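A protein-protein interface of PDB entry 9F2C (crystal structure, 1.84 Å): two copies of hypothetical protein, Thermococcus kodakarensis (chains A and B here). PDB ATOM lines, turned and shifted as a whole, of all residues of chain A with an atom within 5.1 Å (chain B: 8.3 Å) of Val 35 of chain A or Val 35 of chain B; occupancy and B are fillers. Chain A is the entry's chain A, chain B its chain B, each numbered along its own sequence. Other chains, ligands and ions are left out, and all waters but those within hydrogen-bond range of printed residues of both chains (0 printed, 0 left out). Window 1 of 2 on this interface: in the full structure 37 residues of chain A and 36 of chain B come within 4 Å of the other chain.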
ATOM      1  N   MET A   4     -20.221  15.456  24.055  1.00  0.00           N
ATOM      2  CA  MET A   4     -21.483  15.280  23.296  1.00  0.00           C
ATOM      3  C   MET A   4     -21.210  14.607  21.945  1.00  0.00           C
ATOM      4  O   MET A   4     -22.149  14.006  21.407  1.00  0.00           O
ATOM      5  CB  MET A   4     -22.167  16.631  23.074  1.00  0.00           C
ATOM      6  CG  MET A   4     -22.805  17.184  24.341  1.00  0.00           C
ATOM      7  SD  MET A   4     -23.532  18.804  24.080  1.00  0.00           S
ATOM      8  CE  MET A   4     -22.074  19.834  24.216  1.00  0.00           C
ATOM      9  N   LEU A   5     -19.982  14.676  21.429  1.00  0.00           N
ATOM     10  CA  LEU A   5     -19.654  14.205  20.052  1.00  0.00           C
ATOM     11  C   LEU A   5     -19.061  12.798  20.108  1.00  0.00           C
ATOM     12  O   LEU A   5     -18.371  12.481  21.101  1.00  0.00           O
ATOM     13  CB  LEU A   5     -18.662  15.165  19.388  1.00  0.00           C
ATOM     14  CG  LEU A   5     -19.200  16.548  19.030  1.00  0.00           C
ATOM     15  CD1 LEU A   5     -18.063  17.444  18.553  1.00  0.00           C
ATOM     16  CD2 LEU A   5     -20.305  16.487  17.975  1.00  0.00           C
ATOM     17  N   LEU A  31     -13.915  21.311  18.179  1.00  0.00           N
ATOM     18  CA  LEU A  31     -15.301  21.117  17.675  1.00  0.00           C
ATOM     19  C   LEU A  31     -16.245  20.907  18.870  1.00  0.00           C
ATOM     20  O   LEU A  31     -17.321  21.560  18.888  1.00  0.00           O
ATOM     21  CB  LEU A  31     -15.376  19.948  16.698  1.00  0.00           C
ATOM     22  CG  LEU A  31     -16.773  19.687  16.119  1.00  0.00           C
ATOM     23  CD1 LEU A  31     -17.254  20.866  15.287  1.00  0.00           C
ATOM     24  CD2 LEU A  31     -16.777  18.432  15.284  1.00  0.00           C
ATOM     25  N   GLU A  32     -15.838  20.079  19.836  1.00  0.00           N
ATOM     26  CA  GLU A  32     -16.618  19.808  21.073  1.00  0.00           C
ATOM     27  C   GLU A  32     -16.878  21.138  21.801  1.00  0.00           C
ATOM     28  O   GLU A  32     -18.027  21.367  22.205  1.00  0.00           O
ATOM     29  CB  GLU A  32     -15.885  18.779  21.941  1.00  0.00           C
ATOM     30  CG  GLU A  32     -16.600  18.441  23.244  1.00  0.00           C
ATOM     31  CD  GLU A  32     -17.865  17.604  23.117  1.00  0.00           C
ATOM     32  OE1 GLU A  32     -18.852  17.897  23.846  1.00  0.00           O
ATOM     33  OE2 GLU A  32     -17.863  16.648  22.325  1.00  0.00           O
ATOM     34  N   ALA A  33     -15.861  21.993  21.952  1.00  0.00           N
ATOM     35  CA  ALA A  33     -15.986  23.299  22.644  1.00  0.00           C
ATOM     36  C   ALA A  33     -16.995  24.181  21.894  1.00  0.00           C
ATOM     37  O   ALA A  33     -17.801  24.852  22.564  1.00  0.00           O
ATOM     38  CB  ALA A  33     -14.643  23.974  22.784  1.00  0.00           C
ATOM     39  N   GLU A  34     -16.976  24.182  20.560  1.00  0.00           N
ATOM     40  CA  GLU A  34     -17.892  25.031  19.752  1.00  0.00           C
ATOM     41  C   GLU A  34     -19.331  24.521  19.897  1.00  0.00           C
ATOM     42  O   GLU A  34     -20.255  25.361  19.966  1.00  0.00           O
ATOM     43  CB  GLU A  34     -17.460  25.087  18.287  1.00  0.00           C
ATOM     44  CG  GLU A  34     -18.083  26.237  17.491  1.00  0.00           C
ATOM     45  CD  GLU A  34     -18.347  27.568  18.199  1.00  0.00           C
ATOM     46  OE1 GLU A  34     -19.483  28.093  18.059  1.00  0.00           O
ATOM     47  OE2 GLU A  34     -17.453  28.067  18.920  1.00  0.00           O
ATOM     48  N   VAL A  35     -19.524  23.203  19.974  1.00  0.00           N
ATOM     49  CA  VAL A  35     -20.883  22.623  20.174  1.00  0.00           C
ATOM     50  C   VAL A  35     -21.401  23.047  21.557  1.00  0.00           C
ATOM     51  O   VAL A  35     -22.566  23.468  21.641  1.00  0.00           O
ATOM     52  CB  VAL A  35     -20.894  21.095  19.993  1.00  0.00           C
ATOM     53  CG1 VAL A  35     -22.261  20.511  20.323  1.00  0.00           C
ATOM     54  CG2 VAL A  35     -20.453  20.707  18.585  1.00  0.00           C
ATOM     55  N   LYS A  36     -20.562  22.983  22.588  1.00  0.00           N
ATOM     56  CA  LYS A  36     -20.914  23.473  23.952  1.00  0.00           C
ATOM     57  C   LYS A  36     -21.325  24.944  23.862  1.00  0.00           C
ATOM     58  O   LYS A  36     -22.339  25.298  24.476  1.00  0.00           O
ATOM     59  CB  LYS A  36     -19.765  23.260  24.942  1.00  0.00           C
ATOM     60  CG  LYS A  36     -19.571  21.826  25.411  1.00  0.00           C
ATOM     61  CD  LYS A  36     -18.508  21.681  26.484  1.00  0.00           C
ATOM     62  CE  LYS A  36     -18.505  20.318  27.142  1.00  0.00           C
ATOM     63  NZ  LYS A  36     -17.941  19.273  26.256  1.00  0.00           N
ATOM     64  N   ALA A  37     -20.579  25.774  23.129  1.00  0.00           N
ATOM     65  CA  ALA A  37     -20.865  27.217  22.956  1.00  0.00           C
ATOM     66  C   ALA A  37     -22.232  27.400  22.280  1.00  0.00           C
ATOM     67  O   ALA A  37     -23.001  28.282  22.732  1.00  0.00           O
ATOM     68  CB  ALA A  37     -19.758  27.900  22.180  1.00  0.00           C
ATOM     69  N   LEU A  38     -22.537  26.619  21.243  1.00  0.00           N
ATOM     70  CA  LEU A  38     -23.858  26.676  20.555  1.00  0.00           C
ATOM     71  C   LEU A  38     -24.972  26.341  21.550  1.00  0.00           C
ATOM     72  O   LEU A  38     -26.006  27.021  21.543  1.00  0.00           O
ATOM     73  CB  LEU A  38     -23.897  25.709  19.368  1.00  0.00           C
ATOM     74  CG  LEU A  38     -23.149  26.177  18.118  1.00  0.00           C
ATOM     75  CD1 LEU A  38     -23.179  25.100  17.048  1.00  0.00           C
ATOM     76  CD2 LEU A  38     -23.729  27.475  17.569  1.00  0.00           C
ATOM     77  N   VAL A  39     -24.792  25.304  22.362  1.00  0.00           N
ATOM     78  CA  VAL A  39     -25.845  24.850  23.316  1.00  0.00           C
ATOM     79  C   VAL A  39     -26.004  25.907  24.416  1.00  0.00           C
ATOM     80  O   VAL A  39     -27.146  26.174  24.800  1.00  0.00           O
ATOM     81  CB  VAL A  39     -25.541  23.448  23.873  1.00  0.00           C
ATOM     82  CG1 VAL A  39     -26.472  23.062  25.012  1.00  0.00           C
ATOM     83  CG2 VAL A  39     -25.583  22.415  22.749  1.00  0.00           C
ATOM     84  N   GLU A  40     -24.914  26.496  24.898  1.00  0.00           N
ATOM     85  CA  GLU A  40     -24.973  27.541  25.954  1.00  0.00           C
ATOM     86  C   GLU A  40     -25.736  28.752  25.405  1.00  0.00           C
ATOM     87  O   GLU A  40     -26.563  29.323  26.152  1.00  0.00           O
ATOM     88  CB  GLU A  40     -23.571  27.866  26.466  1.00  0.00           C
ATOM     89  CG  GLU A  40     -23.036  26.765  27.369  1.00  0.00           C
ATOM     90  CD  GLU A  40     -21.700  27.027  28.040  1.00  0.00           C
ATOM     91  OE1 GLU A  40     -21.697  27.440  29.232  1.00  0.00           O
ATOM     92  OE2 GLU A  40     -20.675  26.774  27.393  1.00  0.00           O
ATOM     93  N   GLU B   3     -24.973  10.272  12.610  1.00  0.00           N
ATOM     94  CA  GLU B   3     -25.206  11.113  13.826  1.00  0.00           C
ATOM     95  C   GLU B   3     -23.892  11.246  14.606  1.00  0.00           C
ATOM     96  O   GLU B   3     -23.356  10.216  15.067  1.00  0.00           O
ATOM     97  CB  GLU B   3     -26.298  10.519  14.718  1.00  0.00           C
ATOM     98  N   MET B   4     -23.395  12.477  14.755  1.00  0.00           N
ATOM     99  CA  MET B   4     -22.137  12.789  15.475  1.00  0.00           C
ATOM    100  C   MET B   4     -22.419  13.015  16.969  1.00  0.00           C
ATOM    101  O   MET B   4     -21.474  12.899  17.749  1.00  0.00           O
ATOM    102  CB  MET B   4     -21.467  14.021  14.857  1.00  0.00           C
ATOM    103  CG  MET B   4     -20.793  13.705  13.530  1.00  0.00           C
ATOM    104  SD  MET B   4     -20.110  15.170  12.717  1.00  0.00           S
ATOM    105  CE  MET B   4     -21.564  15.884  11.958  1.00  0.00           C
ATOM    106  N   LEU B   5     -23.659  13.333  17.355  1.00  0.00           N
ATOM    107  CA  LEU B   5     -24.011  13.674  18.760  1.00  0.00           C
ATOM    108  C   LEU B   5     -24.542  12.461  19.526  1.00  0.00           C
ATOM    109  O   LEU B   5     -25.193  11.632  18.910  1.00  0.00           O
ATOM    110  CB  LEU B   5     -25.043  14.806  18.764  1.00  0.00           C
ATOM    111  CG  LEU B   5     -24.483  16.170  18.364  1.00  0.00           C
ATOM    112  CD1 LEU B   5     -25.590  17.143  18.111  1.00  0.00           C
ATOM    113  CD2 LEU B   5     -23.551  16.717  19.424  1.00  0.00           C
ATOM    114  N   VAL B  10     -25.860  15.349  25.427  1.00  0.00           N
ATOM    115  CA  VAL B  10     -26.388  16.724  25.197  1.00  0.00           C
ATOM    116  C   VAL B  10     -27.332  17.052  26.356  1.00  0.00           C
ATOM    117  O   VAL B  10     -27.159  18.130  26.952  1.00  0.00           O
ATOM    118  CB  VAL B  10     -27.065  16.858  23.826  1.00  0.00           C
ATOM    119  CG1 VAL B  10     -27.758  18.203  23.669  1.00  0.00           C
ATOM    120  CG2 VAL B  10     -26.077  16.633  22.685  1.00  0.00           C
ATOM    121  N   PHE B  13     -25.342  17.663  29.516  1.00  0.00           N
ATOM    122  CA  PHE B  13     -24.637  18.969  29.425  1.00  0.00           C
ATOM    123  C   PHE B  13     -25.629  20.104  29.718  1.00  0.00           C
ATOM    124  O   PHE B  13     -25.309  21.004  30.509  1.00  0.00           O
ATOM    125  CB  PHE B  13     -23.984  19.194  28.062  1.00  0.00           C
ATOM    126  CG  PHE B  13     -23.293  20.532  27.986  1.00  0.00           C
ATOM    127  CD1 PHE B  13     -22.149  20.776  28.732  1.00  0.00           C
ATOM    128  CD2 PHE B  13     -23.830  21.571  27.238  1.00  0.00           C
ATOM    129  CE1 PHE B  13     -21.535  22.021  28.697  1.00  0.00           C
ATOM    130  CE2 PHE B  13     -23.216  22.814  27.213  1.00  0.00           C
ATOM    131  CZ  PHE B  13     -22.066  23.035  27.931  1.00  0.00           C
ATOM    132  N   PHE B  27     -34.746  19.661  18.827  1.00  0.00           N
ATOM    133  CA  PHE B  27     -33.513  20.421  19.152  1.00  0.00           C
ATOM    134  C   PHE B  27     -32.287  19.587  18.791  1.00  0.00           C
ATOM    135  O   PHE B  27     -31.346  20.127  18.180  1.00  0.00           O
ATOM    136  CB  PHE B  27     -33.453  20.840  20.623  1.00  0.00           C
ATOM    137  CG  PHE B  27     -32.176  21.567  20.952  1.00  0.00           C
ATOM    138  CD1 PHE B  27     -32.055  22.924  20.681  1.00  0.00           C
ATOM    139  CD2 PHE B  27     -31.066  20.892  21.436  1.00  0.00           C
ATOM    140  CE1 PHE B  27     -30.876  23.604  20.955  1.00  0.00           C
ATOM    141  CE2 PHE B  27     -29.889  21.574  21.704  1.00  0.00           C
ATOM    142  CZ  PHE B  27     -29.795  22.923  21.464  1.00  0.00           C
ATOM    143  N   TYR B  28     -32.282  18.302  19.151  1.00  0.00           N
ATOM    144  CA  TYR B  28     -31.147  17.384  18.855  1.00  0.00           C
ATOM    145  C   TYR B  28     -30.888  17.361  17.346  1.00  0.00           C
ATOM    146  O   TYR B  28     -29.718  17.438  16.954  1.00  0.00           O
ATOM    147  CB  TYR B  28     -31.393  15.959  19.359  1.00  0.00           C
ATOM    148  CG  TYR B  28     -31.572  15.842  20.848  1.00  0.00           C
ATOM    149  CD1 TYR B  28     -30.508  16.005  21.718  1.00  0.00           C
ATOM    150  CD2 TYR B  28     -32.783  15.440  21.377  1.00  0.00           C
ATOM    151  CE1 TYR B  28     -30.681  15.868  23.086  1.00  0.00           C
ATOM    152  CE2 TYR B  28     -32.959  15.268  22.744  1.00  0.00           C
ATOM    153  CZ  TYR B  28     -31.888  15.436  23.599  1.00  0.00           C
ATOM    154  OH  TYR B  28     -32.003  15.299  24.955  1.00  0.00           O
ATOM    155  N   ASP B  29     -31.937  17.275  16.530  1.00  0.00           N
ATOM    156  CA  ASP B  29     -31.851  17.207  15.044  1.00  0.00           C
ATOM    157  C   ASP B  29     -31.263  18.533  14.522  1.00  0.00           C
ATOM    158  O   ASP B  29     -30.366  18.495  13.630  1.00  0.00           O
ATOM    159  CB  ASP B  29     -33.227  16.924  14.433  1.00  0.00           C
ATOM    160  CG  ASP B  29     -33.281  15.913  13.313  1.00  0.00           C
ATOM    161  OD1 ASP B  29     -32.461  14.980  13.347  1.00  0.00           O
ATOM    162  OD2 ASP B  29     -34.189  16.043  12.454  1.00  0.00           O
ATOM    163  N   ALA B  30     -31.744  19.669  15.030  1.00  0.00           N
ATOM    164  CA  ALA B  30     -31.261  21.006  14.612  1.00  0.00           C
ATOM    165  C   ALA B  30     -29.788  21.174  15.032  1.00  0.00           C
ATOM    166  O   ALA B  30     -28.989  21.726  14.246  1.00  0.00           O
ATOM    167  CB  ALA B  30     -32.145  22.080  15.192  1.00  0.00           C
ATOM    168  N   LEU B  31     -29.427  20.708  16.227  1.00  0.00           N
ATOM    169  CA  LEU B  31     -28.030  20.801  16.736  1.00  0.00           C
ATOM    170  C   LEU B  31     -27.117  19.940  15.857  1.00  0.00           C
ATOM    171  O   LEU B  31     -26.023  20.390  15.508  1.00  0.00           O
ATOM    172  CB  LEU B  31     -27.960  20.371  18.200  1.00  0.00           C
ATOM    173  CG  LEU B  31     -26.568  20.471  18.830  1.00  0.00           C
ATOM    174  CD1 LEU B  31     -26.085  21.926  18.837  1.00  0.00           C
ATOM    175  CD2 LEU B  31     -26.563  19.880  20.247  1.00  0.00           C
ATOM    176  N   GLU B  32     -27.560  18.741  15.496  1.00  0.00           N
ATOM    177  CA  GLU B  32     -26.809  17.811  14.606  1.00  0.00           C
ATOM    178  C   GLU B  32     -26.533  18.513  13.273  1.00  0.00           C
ATOM    179  O   GLU B  32     -25.378  18.431  12.786  1.00  0.00           O
ATOM    180  CB  GLU B  32     -27.593  16.505  14.443  1.00  0.00           C
ATOM    181  CG  GLU B  32     -26.900  15.475  13.580  1.00  0.00           C
ATOM    182  CD  GLU B  32     -25.692  14.806  14.215  1.00  0.00           C
ATOM    183  OE1 GLU B  32     -24.739  14.565  13.456  1.00  0.00           O
ATOM    184  OE2 GLU B  32     -25.724  14.487  15.451  1.00  0.00           O
ATOM    185  N   ALA B  33     -27.524  19.193  12.689  1.00  0.00           N
ATOM    186  CA  ALA B  33     -27.360  19.934  11.413  1.00  0.00           C
ATOM    187  C   ALA B  33     -26.307  21.042  11.582  1.00  0.00           C
ATOM    188  O   ALA B  33     -25.493  21.234  10.668  1.00  0.00           O
ATOM    189  CB  ALA B  33     -28.684  20.470  10.934  1.00  0.00           C
ATOM    190  N   GLU B  34     -26.309  21.751  12.713  1.00  0.00           N
ATOM    191  CA  GLU B  34     -25.345  22.854  12.982  1.00  0.00           C
ATOM    192  C   GLU B  34     -23.923  22.280  13.113  1.00  0.00           C
ATOM    193  O   GLU B  34     -22.978  22.923  12.618  1.00  0.00           O
ATOM    194  CB  GLU B  34     -25.718  23.633  14.251  1.00  0.00           C
ATOM    195  CG  GLU B  34     -26.927  24.517  14.101  1.00  0.00           C
ATOM    196  CD  GLU B  34     -26.821  25.489  12.940  1.00  0.00           C
ATOM    197  OE1 GLU B  34     -25.899  26.337  12.952  1.00  0.00           O
ATOM    198  OE2 GLU B  34     -27.617  25.350  12.001  1.00  0.00           O
ATOM    199  N   VAL B  35     -23.771  21.101  13.721  1.00  0.00           N
ATOM    200  CA  VAL B  35     -22.441  20.448  13.864  1.00  0.00           C
ATOM    201  C   VAL B  35     -21.923  20.086  12.461  1.00  0.00           C
ATOM    202  O   VAL B  35     -20.726  20.367  12.175  1.00  0.00           O
ATOM    203  CB  VAL B  35     -22.485  19.218  14.788  1.00  0.00           C
ATOM    204  CG1 VAL B  35     -21.128  18.526  14.836  1.00  0.00           C
ATOM    205  CG2 VAL B  35     -22.964  19.561  16.184  1.00  0.00           C
ATOM    206  N   LYS B  36     -22.787  19.525  11.609  1.00  0.00           N
ATOM    207  CA  LYS B  36     -22.434  19.215  10.198  1.00  0.00           C
ATOM    208  C   LYS B  36     -21.964  20.506   9.510  1.00  0.00           C
ATOM    209  O   LYS B  36     -20.917  20.461   8.826  1.00  0.00           O
ATOM    210  CB  LYS B  36     -23.605  18.576   9.446  1.00  0.00           C
ATOM    211  CG  LYS B  36     -23.879  17.115   9.781  1.00  0.00           C
ATOM    212  CD  LYS B  36     -24.880  16.462   8.844  1.00  0.00           C
ATOM    213  N   ALA B  37     -22.693  21.614   9.697  1.00  0.00           N
ATOM    214  CA  ALA B  37     -22.367  22.925   9.093  1.00  0.00           C
ATOM    215  C   ALA B  37     -20.994  23.404   9.590  1.00  0.00           C
ATOM    216  O   ALA B  37     -20.226  23.904   8.744  1.00  0.00           O
ATOM    217  CB  ALA B  37     -23.445  23.946   9.394  1.00  0.00           C
ATOM    218  N   LEU B  38     -20.689  23.271  10.891  1.00  0.00           N
ATOM    219  CA  LEU B  38     -19.368  23.652  11.461  1.00  0.00           C
ATOM    220  C   LEU B  38     -18.267  22.853  10.757  1.00  0.00           C
ATOM    221  O   LEU B  38     -17.241  23.458  10.390  1.00  0.00           O
ATOM    222  CB  LEU B  38     -19.311  23.385  12.969  1.00  0.00           C
ATOM    223  CG  LEU B  38     -20.053  24.370  13.869  1.00  0.00           C
ATOM    224  CD1 LEU B  38     -20.016  23.893  15.312  1.00  0.00           C
ATOM    225  CD2 LEU B  38     -19.462  25.768  13.747  1.00  0.00           C
ATOM    226  N   VAL B  39     -18.458  21.545  10.601  1.00  0.00           N
ATOM    227  CA  VAL B  39     -17.396  20.670  10.027  1.00  0.00           C
ATOM    228  C   VAL B  39     -17.220  21.014   8.538  1.00  0.00           C
ATOM    229  O   VAL B  39     -16.045  21.073   8.073  1.00  0.00           O
ATOM    230  CB  VAL B  39     -17.701  19.182  10.263  1.00  0.00           C
ATOM    231  CG1 VAL B  39     -16.706  18.291   9.517  1.00  0.00           C
ATOM    232  CG2 VAL B  39     -17.713  18.861  11.752  1.00  0.00           C
ATOM    233  N   GLU B  40     -18.328  21.241   7.816  1.00  0.00           N
ATOM    234  CA  GLU B  40     -18.268  21.576   6.372  1.00  0.00           C
ATOM    235  C   GLU B  40     -17.507  22.903   6.209  1.00  0.00           C
ATOM    236  O   GLU B  40     -16.672  22.994   5.286  1.00  0.00           O
ATOM    237  CB  GLU B  40     -19.671  21.617   5.759  1.00  0.00           C
ATOM    238  CG  GLU B  40     -20.333  20.263   5.611  1.00  0.00           C
ATOM    239  CD  GLU B  40     -21.847  20.316   5.403  1.00  0.00           C
ATOM    240  OE1 GLU B  40     -22.446  21.410   5.579  1.00  0.00           O
ATOM    241  OE2 GLU B  40     -22.448  19.267   5.076  1.00  0.00           O
ATOM    242  N   LYS B  41     -17.757  23.879   7.092  1.00  0.00           N
ATOM    243  CA  LYS B  41     -17.090  25.202   7.034  1.00  0.00           C
ATOM    244  C   LYS B  41     -15.599  25.016   7.334  1.00  0.00           C
ATOM    245  O   LYS B  41     -14.784  25.618   6.619  1.00  0.00           O
ATOM    246  CB  LYS B  41     -17.731  26.226   7.978  1.00  0.00           C
ATOM    247  CG  LYS B  41     -17.488  27.676   7.555  1.00  0.00           C
ATOM    248  CD  LYS B  41     -18.590  28.690   7.804  1.00  0.00           C
ATOM    249  CE  LYS B  41     -18.200  30.044   7.234  1.00  0.00           C
ATOM    250  NZ  LYS B  41     -18.870  31.184   7.911  1.00  0.00           N
ATOM    251  N   ALA B  42     -15.256  24.215   8.339  1.00  0.00           N
ATOM    252  CA  ALA B  42     -13.849  23.908   8.707  1.00  0.00           C
ATOM    253  C   ALA B  42     -13.116  23.318   7.493  1.00  0.00           C
ATOM    254  O   ALA B  42     -11.981  23.753   7.195  1.00  0.00           O
ATOM    255  CB  ALA B  42     -13.808  22.972   9.887  1.00  0.00           C
ATOM    256  N   VAL B  59     -11.986  25.358  12.964  1.00  0.00           N
ATOM    257  CA  VAL B  59     -13.351  25.267  13.574  1.00  0.00           C
ATOM    258  C   VAL B  59     -13.939  26.673  13.684  1.00  0.00           C
ATOM    259  O   VAL B  59     -13.246  27.637  14.038  1.00  0.00           O
ATOM    260  CB  VAL B  59     -13.337  24.580  14.953  1.00  0.00           C
ATOM    261  CG1 VAL B  59     -14.670  24.736  15.677  1.00  0.00           C
ATOM    262  CG2 VAL B  59     -12.950  23.120  14.852  1.00  0.00           C
ATOM    263  OXT VAL B  59     -15.134  26.841  13.429  1.00  0.00           O
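Along chain B the printed residues that touch a printed residue of chain A span positions 4 to 59. Hydrophobic or aromatic side chains of chain A within 4 Å of the printed part of chain B: Met 4, Leu 5, Leu 31, Val 35, Leu 38 and Val 39. Along chain A the printed residues that touch a printed residue of chain B span positions 4 to 40. Among the printed residues, 18 pairs touch across the chains. Among the printed residues, no Asp or Glu carboxylate lies within 4 Å of a Lys or Arg side-chain nitrogen of the other chain.
Met 4 of chain B touches its own counterpart, Met 4 of chain A. Leu 5 of chain A touches its own counterpart, Leu 5 of chain B. Val 35 of chain B touches its own counterpart, Val 35 of chain A. Leu 38 of chain A touches its own counterpart, Leu 38 of chain B. Positions printed for both chains: 4, 5, 31, 32, 33, 34, 35, 36, 37, 38, 39 and 40. Of the 18 pairs that touch across the chains among the printed residues, 8 have their exchanged pair printed and touching as well.
Of the printed residues of chain B, Val 35 of chain A touches Val 35. Val 35 of chain B touches just these residues of chain A: Leu 5 and Val 35. Of the printed residues of chain A, Leu 5 of chain B touches Met 4 and Leu 5. Of the printed residues of chain A, Val 10 of chain B touches Met 4 (3.6 Å). Of the printed residues of chain A, Phe 13 of chain B touches Met 4 (3.9 Å), Lys 36 (3.7 Å), Val 39 (3.8 Å) and Glu 40 (3.9 Å). Lys 41 of chain B touches none of the printed residues of chain A. The nearest residue of chain A that does not touch Val 35 of chain B is Leu 31 of chain A (4.4 Å).
Among the printed residues, merely in contact across the chains: Met 4 of chain A with Met 4 of chain B (3.9 Å), Met 4 of chain A with Leu 5 of chain B (3.3 Å), Met 4 of chain A with Val 10 of chain B (3.6 Å), Met 4 of chain A with Phe 13 of chain B (3.9 Å), Leu 5 of chain A with Met 4 of chain B (3.2 Å), Leu 5 of chain A with Leu 5 of chain B (3.6 Å), Leu 5 of chain A with Val 35 of chain B (3.8 Å), Leu 31 of chain A with Leu 38 of chain B (3.99 Å), Leu 31 of chain A with Val 39 of chain B (3.7 Å), Leu 31 of chain A with Val 59 of chain B (3.9 Å), Glu 34 of chain A with Leu 38 of chain B (3.7 Å), Glu 34 of chain A with Val 59 of chain B (3.8 Å), Val 35 of chain A with Val 35 of chain B (3.7 Å), Lys 36 of chain A with Phe 13 of chain B (3.7 Å), Leu 38 of chain A with Leu 38 of chain B (3.8 Å), Val 39 of chain A with Phe 13 of chain B (3.8 Å), Val 39 of chain A with Leu 31 of chain B (3.7 Å) and Glu 40 of chain A with Phe 13 of chain B (3.9 Å).
OE1 of Glu 32 of chain A is in salt-bridge range of NZ of Lys 36 of chain A (2.9 Å). The backbone NH of Leu 5 of chain B lies within hydrogen-bond range of the side-chain carboxylate of Glu 32 of chain B, 3.0 Å away. N of Met 4 of chain A is in hydrogen-bond range of OE1 of Glu 32 of chain A (2.8 Å). The backbone NH (N) of Leu 5 of chain A lies within hydrogen-bond range of the side-chain carboxylate (OE2) of Glu 32 of chain A, 3.0 Å away. The side-chain carboxylate (OE1) of Glu 32 of chain B lies within hydrogen-bond range of the backbone NH (N) of Met 4 of chain B (2.8 Å).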
